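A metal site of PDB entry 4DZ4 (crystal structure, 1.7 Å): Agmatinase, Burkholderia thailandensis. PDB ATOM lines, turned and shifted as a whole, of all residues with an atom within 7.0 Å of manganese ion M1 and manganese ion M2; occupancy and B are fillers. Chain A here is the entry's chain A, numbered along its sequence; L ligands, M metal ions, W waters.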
ATOM      1  N   ASP A 138      -1.749  12.641 -23.012  1.00  0.00           N
ATOM      2  CA  ASP A 138      -2.564  12.422 -21.821  1.00  0.00           C
ATOM      3  C   ASP A 138      -4.037  12.674 -22.080  1.00  0.00           C
ATOM      4  O   ASP A 138      -4.426  13.183 -23.153  1.00  0.00           O
ATOM      5  CB  ASP A 138      -2.027  13.192 -20.594  1.00  0.00           C
ATOM      6  CG  ASP A 138      -2.286  14.715 -20.649  1.00  0.00           C
ATOM      7  OD1 ASP A 138      -3.419  15.145 -20.979  1.00  0.00           O
ATOM      8  OD2 ASP A 138      -1.350  15.496 -20.323  1.00  0.00           O
ATOM      9  N   HIS A 139      -4.878  12.258 -21.130  1.00  0.00           N
ATOM     10  CA  HIS A 139      -6.316  12.217 -21.379  1.00  0.00           C
ATOM     11  C   HIS A 139      -6.924  13.572 -21.549  1.00  0.00           C
ATOM     12  O   HIS A 139      -8.062  13.696 -22.035  1.00  0.00           O
ATOM     13  CB  HIS A 139      -7.029  11.435 -20.292  1.00  0.00           C
ATOM     14  CG  HIS A 139      -8.164  10.587 -20.806  1.00  0.00           C
ATOM     15  ND1 HIS A 139      -8.665   9.537 -20.114  1.00  0.00           N
ATOM     16  CD2 HIS A 139      -8.879  10.664 -21.985  1.00  0.00           C
ATOM     17  CE1 HIS A 139      -9.633   8.960 -20.828  1.00  0.00           C
ATOM     18  NE2 HIS A 139      -9.770   9.650 -21.987  1.00  0.00           N
ATOM     19  N   TYR A 140      -6.222  14.622 -21.147  1.00  0.00           N
ATOM     20  CA  TYR A 140      -6.806  15.958 -21.254  1.00  0.00           C
ATOM     21  C   TYR A 140      -7.145  16.244 -22.727  1.00  0.00           C
ATOM     22  O   TYR A 140      -8.118  16.961 -23.023  1.00  0.00           O
ATOM     23  CB  TYR A 140      -5.903  17.053 -20.669  1.00  0.00           C
ATOM     24  CG  TYR A 140      -6.465  18.460 -20.931  1.00  0.00           C
ATOM     25  CD1 TYR A 140      -7.407  19.032 -20.076  1.00  0.00           C
ATOM     26  CD2 TYR A 140      -6.097  19.177 -22.083  1.00  0.00           C
ATOM     27  CE1 TYR A 140      -7.923  20.306 -20.332  1.00  0.00           C
ATOM     28  CE2 TYR A 140      -6.627  20.443 -22.366  1.00  0.00           C
ATOM     29  CZ  TYR A 140      -7.546  21.005 -21.483  1.00  0.00           C
ATOM     30  OH  TYR A 140      -8.068  22.276 -21.745  1.00  0.00           O
ATOM     31  N   HIS A 161     -16.104   5.437 -22.577  1.00  0.00           N
ATOM     32  CA  HIS A 161     -14.843   5.808 -21.925  1.00  0.00           C
ATOM     33  C   HIS A 161     -14.274   4.597 -21.215  1.00  0.00           C
ATOM     34  O   HIS A 161     -14.891   4.087 -20.267  1.00  0.00           O
ATOM     35  CB  HIS A 161     -15.193   6.991 -21.000  1.00  0.00           C
ATOM     36  CG  HIS A 161     -14.093   7.461 -20.089  1.00  0.00           C
ATOM     37  ND1 HIS A 161     -14.373   8.165 -18.953  1.00  0.00           N
ATOM     38  CD2 HIS A 161     -12.711   7.322 -20.137  1.00  0.00           C
ATOM     39  CE1 HIS A 161     -13.235   8.477 -18.325  1.00  0.00           C
ATOM     40  NE2 HIS A 161     -12.207   7.983 -19.050  1.00  0.00           N
ATOM     41  N   PHE A 162     -13.140   4.094 -21.705  1.00  0.00           N
ATOM     42  CA  PHE A 162     -12.401   2.970 -21.083  1.00  0.00           C
ATOM     43  C   PHE A 162     -11.271   3.562 -20.239  1.00  0.00           C
ATOM     44  O   PHE A 162     -10.461   4.321 -20.763  1.00  0.00           O
ATOM     45  CB  PHE A 162     -11.776   2.077 -22.145  1.00  0.00           C
ATOM     46  CG  PHE A 162     -12.784   1.268 -22.926  1.00  0.00           C
ATOM     47  CD1 PHE A 162     -13.412   1.830 -24.037  1.00  0.00           C
ATOM     48  CD2 PHE A 162     -13.077  -0.050 -22.578  1.00  0.00           C
ATOM     49  CE1 PHE A 162     -14.341   1.082 -24.763  1.00  0.00           C
ATOM     50  CE2 PHE A 162     -14.011  -0.800 -23.296  1.00  0.00           C
ATOM     51  CZ  PHE A 162     -14.632  -0.224 -24.422  1.00  0.00           C
ATOM     52  N   ASP A 163     -11.214   3.226 -18.935  1.00  0.00           N
ATOM     53  CA  ASP A 163     -10.318   3.932 -18.026  1.00  0.00           C
ATOM     54  C   ASP A 163     -10.382   3.332 -16.640  1.00  0.00           C
ATOM     55  O   ASP A 163     -11.432   2.833 -16.217  1.00  0.00           O
ATOM     56  CB  ASP A 163     -10.762   5.405 -17.966  1.00  0.00           C
ATOM     57  CG  ASP A 163      -9.634   6.375 -17.666  1.00  0.00           C
ATOM     58  OD1 ASP A 163      -8.752   6.066 -16.838  1.00  0.00           O
ATOM     59  OD2 ASP A 163      -9.642   7.489 -18.222  1.00  0.00           O
ATOM     60  N   ALA A 164      -9.275   3.379 -15.900  1.00  0.00           N
ATOM     61  CA  ALA A 164      -9.371   3.064 -14.459  1.00  0.00           C
ATOM     62  C   ALA A 164      -9.971   4.247 -13.688  1.00  0.00           C
ATOM     63  O   ALA A 164     -10.401   4.063 -12.553  1.00  0.00           O
ATOM     64  CB  ALA A 164      -7.979   2.764 -13.900  1.00  0.00           C
ATOM     65  N   HIS A 165      -9.955   5.425 -14.335  1.00  0.00           N
ATOM     66  CA  HIS A 165     -10.327   6.708 -13.721  1.00  0.00           C
ATOM     67  C   HIS A 165     -11.520   7.307 -14.420  1.00  0.00           C
ATOM     68  O   HIS A 165     -11.588   7.331 -15.653  1.00  0.00           O
ATOM     69  CB  HIS A 165      -9.184   7.702 -13.871  1.00  0.00           C
ATOM     70  CG  HIS A 165      -7.876   7.174 -13.333  1.00  0.00           C
ATOM     71  ND1 HIS A 165      -6.946   6.576 -14.116  1.00  0.00           N
ATOM     72  CD2 HIS A 165      -7.393   7.114 -12.041  1.00  0.00           C
ATOM     73  CE1 HIS A 165      -5.917   6.157 -13.340  1.00  0.00           C
ATOM     74  NE2 HIS A 165      -6.183   6.508 -12.074  1.00  0.00           N
ATOM     75  N   CYS A 166     -12.437   7.834 -13.612  1.00  0.00           N
ATOM     76  CA  CYS A 166     -13.641   8.455 -14.170  1.00  0.00           C
ATOM     77  C   CYS A 166     -13.368   9.819 -14.819  1.00  0.00           C
ATOM     78  O   CYS A 166     -14.122  10.264 -15.700  1.00  0.00           O
ATOM     79  CB  CYS A 166     -14.718   8.574 -13.083  1.00  0.00           C
ATOM     80  SG  CYS A 166     -14.210   9.656 -11.712  1.00  0.00           S
ATOM     81  N   ASP A 167     -12.296  10.502 -14.382  1.00  0.00           N
ATOM     82  CA  ASP A 167     -11.940  11.856 -14.879  1.00  0.00           C
ATOM     83  C   ASP A 167     -13.092  12.856 -14.776  1.00  0.00           C
ATOM     84  O   ASP A 167     -13.186  13.800 -15.571  1.00  0.00           O
ATOM     85  CB  ASP A 167     -11.366  11.787 -16.297  1.00  0.00           C
ATOM     86  CG  ASP A 167     -10.171  10.887 -16.360  1.00  0.00           C
ATOM     87  OD1 ASP A 167      -9.497  10.687 -15.305  1.00  0.00           O
ATOM     88  OD2 ASP A 167      -9.876  10.346 -17.430  1.00  0.00           O
ATOM     89  N   TRP A 169     -13.830  14.191 -11.570  1.00  0.00           N
ATOM     90  CA  TRP A 169     -13.666  14.899 -10.285  1.00  0.00           C
ATOM     91  C   TRP A 169     -13.938  16.366 -10.499  1.00  0.00           C
ATOM     92  O   TRP A 169     -13.549  16.909 -11.549  1.00  0.00           O
ATOM     93  CB  TRP A 169     -12.273  14.632  -9.714  1.00  0.00           C
ATOM     94  CG  TRP A 169     -12.136  13.175  -9.314  1.00  0.00           C
ATOM     95  CD1 TRP A 169     -12.666  12.569  -8.173  1.00  0.00           C
ATOM     96  CD2 TRP A 169     -11.465  12.082 -10.053  1.00  0.00           C
ATOM     97  NE1 TRP A 169     -12.369  11.229  -8.132  1.00  0.00           N
ATOM     98  CE2 TRP A 169     -11.647  10.877  -9.230  1.00  0.00           C
ATOM     99  CE3 TRP A 169     -10.728  11.999 -11.233  1.00  0.00           C
ATOM    100  CZ2 TRP A 169     -11.131   9.636  -9.615  1.00  0.00           C
ATOM    101  CZ3 TRP A 169     -10.219  10.744 -11.603  1.00  0.00           C
ATOM    102  CH2 TRP A 169     -10.415   9.597 -10.811  1.00  0.00           C
ATOM    103  N   HIS A 179      -5.824  16.163 -16.553  1.00  0.00           N
ATOM    104  CA  HIS A 179      -6.355  14.973 -17.234  1.00  0.00           C
ATOM    105  C   HIS A 179      -7.365  14.197 -16.440  1.00  0.00           C
ATOM    106  O   HIS A 179      -7.891  13.204 -16.936  1.00  0.00           O
ATOM    107  CB  HIS A 179      -5.225  14.038 -17.723  1.00  0.00           C
ATOM    108  CG  HIS A 179      -4.458  13.332 -16.605  1.00  0.00           C
ATOM    109  ND1 HIS A 179      -3.699  12.221 -16.838  1.00  0.00           N
ATOM    110  CD2 HIS A 179      -4.347  13.597 -15.245  1.00  0.00           C
ATOM    111  CE1 HIS A 179      -3.125  11.801 -15.684  1.00  0.00           C
ATOM    112  NE2 HIS A 179      -3.518  12.635 -14.697  1.00  0.00           N
ATOM    113  N   GLY A 180      -7.672  14.659 -15.222  1.00  0.00           N
ATOM    114  CA  GLY A 180      -8.621  13.970 -14.353  1.00  0.00           C
ATOM    115  C   GLY A 180      -9.883  14.759 -14.051  1.00  0.00           C
ATOM    116  O   GLY A 180     -10.756  14.299 -13.323  1.00  0.00           O
ATOM    117  N   MET A 182     -11.489  16.771 -16.840  1.00  0.00           N
ATOM    118  CA  MET A 182     -12.031  17.323 -18.084  1.00  0.00           C
ATOM    119  C   MET A 182     -13.404  16.745 -18.458  1.00  0.00           C
ATOM    120  O   MET A 182     -14.156  17.383 -19.196  1.00  0.00           O
ATOM    121  CB  MET A 182     -11.002  17.257 -19.242  1.00  0.00           C
ATOM    122  CG  MET A 182     -10.755  15.860 -19.833  1.00  0.00           C
ATOM    123  SD  MET A 182      -9.694  14.858 -18.793  1.00  0.00           S
ATOM    124  CE  MET A 182     -10.093  13.243 -19.498  1.00  0.00           C
ATOM    125  N   PHE A 183     -13.765  15.578 -17.930  1.00  0.00           N
ATOM    126  CA  PHE A 183     -15.112  15.038 -18.181  1.00  0.00           C
ATOM    127  C   PHE A 183     -16.177  15.578 -17.222  1.00  0.00           C
ATOM    128  O   PHE A 183     -17.370  15.582 -17.555  1.00  0.00           O
ATOM    129  CB  PHE A 183     -15.139  13.508 -18.284  1.00  0.00           C
ATOM    130  CG  PHE A 183     -14.316  12.947 -19.423  1.00  0.00           C
ATOM    131  CD1 PHE A 183     -14.066  13.698 -20.577  1.00  0.00           C
ATOM    132  CD2 PHE A 183     -13.789  11.661 -19.345  1.00  0.00           C
ATOM    133  CE1 PHE A 183     -13.315  13.195 -21.623  1.00  0.00           C
ATOM    134  CE2 PHE A 183     -13.035  11.149 -20.391  1.00  0.00           C
ATOM    135  CZ  PHE A 183     -12.792  11.919 -21.531  1.00  0.00           C
ATOM    136  N   THR A 244     -13.268   6.905 -26.145  1.00  0.00           N
ATOM    137  CA  THR A 244     -11.960   7.347 -25.643  1.00  0.00           C
ATOM    138  C   THR A 244     -11.381   6.222 -24.819  1.00  0.00           C
ATOM    139  O   THR A 244     -12.020   5.724 -23.884  1.00  0.00           O
ATOM    140  CB  THR A 244     -12.062   8.675 -24.858  1.00  0.00           C
ATOM    141  OG1 THR A 244     -10.777   9.029 -24.350  1.00  0.00           O
ATOM    142  CG2 THR A 244     -13.065   8.557 -23.661  1.00  0.00           C
ATOM    143  N   ASP A 246      -8.372   5.093 -22.551  1.00  0.00           N
ATOM    144  CA  ASP A 246      -7.173   5.296 -21.729  1.00  0.00           C
ATOM    145  C   ASP A 246      -6.555   3.937 -21.474  1.00  0.00           C
ATOM    146  O   ASP A 246      -7.218   3.026 -20.964  1.00  0.00           O
ATOM    147  CB  ASP A 246      -7.584   6.000 -20.420  1.00  0.00           C
ATOM    148  CG  ASP A 246      -6.434   6.252 -19.476  1.00  0.00           C
ATOM    149  OD1 ASP A 246      -5.348   5.640 -19.593  1.00  0.00           O
ATOM    150  OD2 ASP A 246      -6.631   7.096 -18.596  1.00  0.00           O
ATOM    151  N   ILE A 247      -5.280   3.792 -21.854  1.00  0.00           N
ATOM    152  CA  ILE A 247      -4.630   2.484 -21.818  1.00  0.00           C
ATOM    153  C   ILE A 247      -4.533   1.973 -20.370  1.00  0.00           C
ATOM    154  O   ILE A 247      -4.432   0.758 -20.154  1.00  0.00           O
ATOM    155  CB  ILE A 247      -3.252   2.486 -22.528  1.00  0.00           C
ATOM    156  CG1 ILE A 247      -2.879   1.074 -23.027  1.00  0.00           C
ATOM    157  CG2 ILE A 247      -2.159   3.127 -21.671  1.00  0.00           C
ATOM    158  CD1 ILE A 247      -3.842   0.455 -24.051  1.00  0.00           C
ATOM    159  N   ASP A 248      -4.631   2.878 -19.394  1.00  0.00           N
ATOM    160  CA  ASP A 248      -4.642   2.404 -17.991  1.00  0.00           C
ATOM    161  C   ASP A 248      -5.927   1.674 -17.551  1.00  0.00           C
ATOM    162  O   ASP A 248      -6.028   1.202 -16.427  1.00  0.00           O
ATOM    163  CB  ASP A 248      -4.204   3.505 -17.007  1.00  0.00           C
ATOM    164  CG  ASP A 248      -5.264   4.586 -16.780  1.00  0.00           C
ATOM    165  OD1 ASP A 248      -6.486   4.326 -16.987  1.00  0.00           O
ATOM    166  OD2 ASP A 248      -4.862   5.694 -16.369  1.00  0.00           O
ATOM    167  N   CYS A 249      -6.901   1.572 -18.467  1.00  0.00           N
ATOM    168  CA  CYS A 249      -8.016   0.659 -18.282  1.00  0.00           C
ATOM    169  C   CYS A 249      -7.483  -0.763 -18.074  1.00  0.00           C
ATOM    170  O   CYS A 249      -7.963  -1.522 -17.217  1.00  0.00           O
ATOM    171  CB  CYS A 249      -8.908   0.717 -19.526  1.00  0.00           C
ATOM    172  SG  CYS A 249     -10.284  -0.456 -19.484  1.00  0.00           S
ATOM    173  N   THR A 258       2.332   3.553 -18.469  1.00  0.00           N
ATOM    174  CA  THR A 258       1.307   4.592 -18.320  1.00  0.00           C
ATOM    175  C   THR A 258       1.589   5.408 -17.079  1.00  0.00           C
ATOM    176  O   THR A 258       2.298   4.932 -16.179  1.00  0.00           O
ATOM    177  CB  THR A 258      -0.092   3.925 -18.353  1.00  0.00           C
ATOM    178  OG1 THR A 258      -1.091   4.926 -18.680  1.00  0.00           O
ATOM    179  CG2 THR A 258      -0.378   3.218 -17.030  1.00  0.00           C
ATOM    180  N   THR A 260      -0.458   6.714 -14.593  1.00  0.00           N
ATOM    181  CA  THR A 260      -1.243   6.489 -13.354  1.00  0.00           C
ATOM    182  C   THR A 260      -1.736   5.034 -13.310  1.00  0.00           C
ATOM    183  O   THR A 260      -2.925   4.758 -13.496  1.00  0.00           O
ATOM    184  CB  THR A 260      -2.448   7.476 -13.233  1.00  0.00           C
ATOM    185  OG1 THR A 260      -3.149   7.523 -14.489  1.00  0.00           O
ATOM    186  CG2 THR A 260      -1.993   8.885 -12.838  1.00  0.00           C
ATOM    187  N   VAL A 262      -3.085   1.510 -11.991  1.00  0.00           N
ATOM    188  CA  VAL A 262      -3.951   1.099 -10.876  1.00  0.00           C
ATOM    189  C   VAL A 262      -4.190  -0.407 -10.952  1.00  0.00           C
ATOM    190  O   VAL A 262      -4.627  -0.913 -11.976  1.00  0.00           O
ATOM    191  CB  VAL A 262      -5.345   1.792 -10.943  1.00  0.00           C
ATOM    192  CG1 VAL A 262      -6.152   1.414  -9.706  1.00  0.00           C
ATOM    193  CG2 VAL A 262      -5.213   3.296 -11.094  1.00  0.00           C
ATOM    194  N   VAL A 289      -5.246   6.905 -25.522  1.00  0.00           N
ATOM    195  CA  VAL A 289      -4.445   7.880 -24.781  1.00  0.00           C
ATOM    196  C   VAL A 289      -3.641   7.247 -23.649  1.00  0.00           C
ATOM    197  O   VAL A 289      -3.890   6.095 -23.265  1.00  0.00           O
ATOM    198  CB  VAL A 289      -5.307   9.033 -24.197  1.00  0.00           C
ATOM    199  CG1 VAL A 289      -6.059   9.757 -25.324  1.00  0.00           C
ATOM    200  CG2 VAL A 289      -6.322   8.483 -23.176  1.00  0.00           C
ATOM    201  N   GLU A 290      -2.691   8.051 -23.162  1.00  0.00           N
ATOM    202  CA  GLU A 290      -1.910   7.775 -21.932  1.00  0.00           C
ATOM    203  C   GLU A 290      -0.795   6.723 -22.093  1.00  0.00           C
ATOM    204  O   GLU A 290      -0.229   6.272 -21.085  1.00  0.00           O
ATOM    205  CB  GLU A 290      -2.808   7.453 -20.707  1.00  0.00           C
ATOM    206  CG  GLU A 290      -3.755   8.562 -20.242  1.00  0.00           C
ATOM    207  CD  GLU A 290      -3.054   9.681 -19.440  1.00  0.00           C
ATOM    208  OE1 GLU A 290      -1.861   9.544 -19.098  1.00  0.00           O
ATOM    209  OE2 GLU A 290      -3.709  10.689 -19.108  1.00  0.00           O
HETATM  210  O1  LIG L   1      -6.870  10.741 -17.316  1.00  0.00           O
HETATM  211  O1  LG2 L   2      -5.042   9.032 -16.110  1.00  0.00           O
HETATM  212 MN    MN M   1      -8.272   9.123 -17.975  1.00  0.00          MN
HETATM  213 MN    MN M   2      -6.780   6.695 -16.414  1.00  0.00          MN
HETATM  214  O   HOH W   1      -7.327   8.717 -16.321  1.00  0.00           O
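Of the 25 residues printed, 4 come within 4 Å of manganese ion M2.
Along chain A the residues within 4 Å of manganese ion M2 span positions 163 to 248.
The nearest printed residue that does not touch manganese ion M2 is Ala 164 (4.2 Å).
Manganese ion M1 is bound by water W1 (1.9 Å), OD2 of Asp 167 (2.1 Å), OD2 of Asp 163 (2.1 Å), ND1 of His 139 (2.2 Å), O1 of LIG L1 (2.2 Å) and OD2 of Asp 246 (2.7 Å).
Manganese ion M1 has six donor atoms within binding distance.
N of Phe 183 sits at hydrogen-bond distance from O of Asp 167 (3.0 Å).
The side-chain carboxylate of Asp 163 lies close to a ring nitrogen (NE2) of His 161.
The backbone NH (N) of Ala 164 lies close to the side-chain carboxylate (OD1) of Asp 248 (3.1 Å).
OD2 of Asp 248 sits close to OG1 of Thr 260 (3.1 Å).
OE2 of Glu 290 lies within hydrogen-bond range of N of His 139, at 2.8 Å.
OG1 of Thr 244 lies within hydrogen-bond range of NE2 of His 139 (2.6 Å).
The backbone NH of Asp 246 lies within hydrogen-bond range of the backbone carbonyl oxygen of Phe 162, 2.9 Å away.
Manganese ion M2 is bound by water W1 (2.1 Å), OD1 of Asp 163 (2.1 Å), OD2 of Asp 248 (2.2 Å), OD2 of Asp 246 (2.2 Å), ND1 of His 165 (2.3 Å) and OD1 of Asp 248 (2.5 Å).
Slightly farther from manganese ion M2 lies O1 of LG2 L2 (2.9 Å).
Four residues have an atom within 4 Å of manganese ion M1: His 139, Asp 163, Asp 167 and Asp 246.
The nearest printed residue that does not touch manganese ion M1 is His 179 (4.2 Å).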
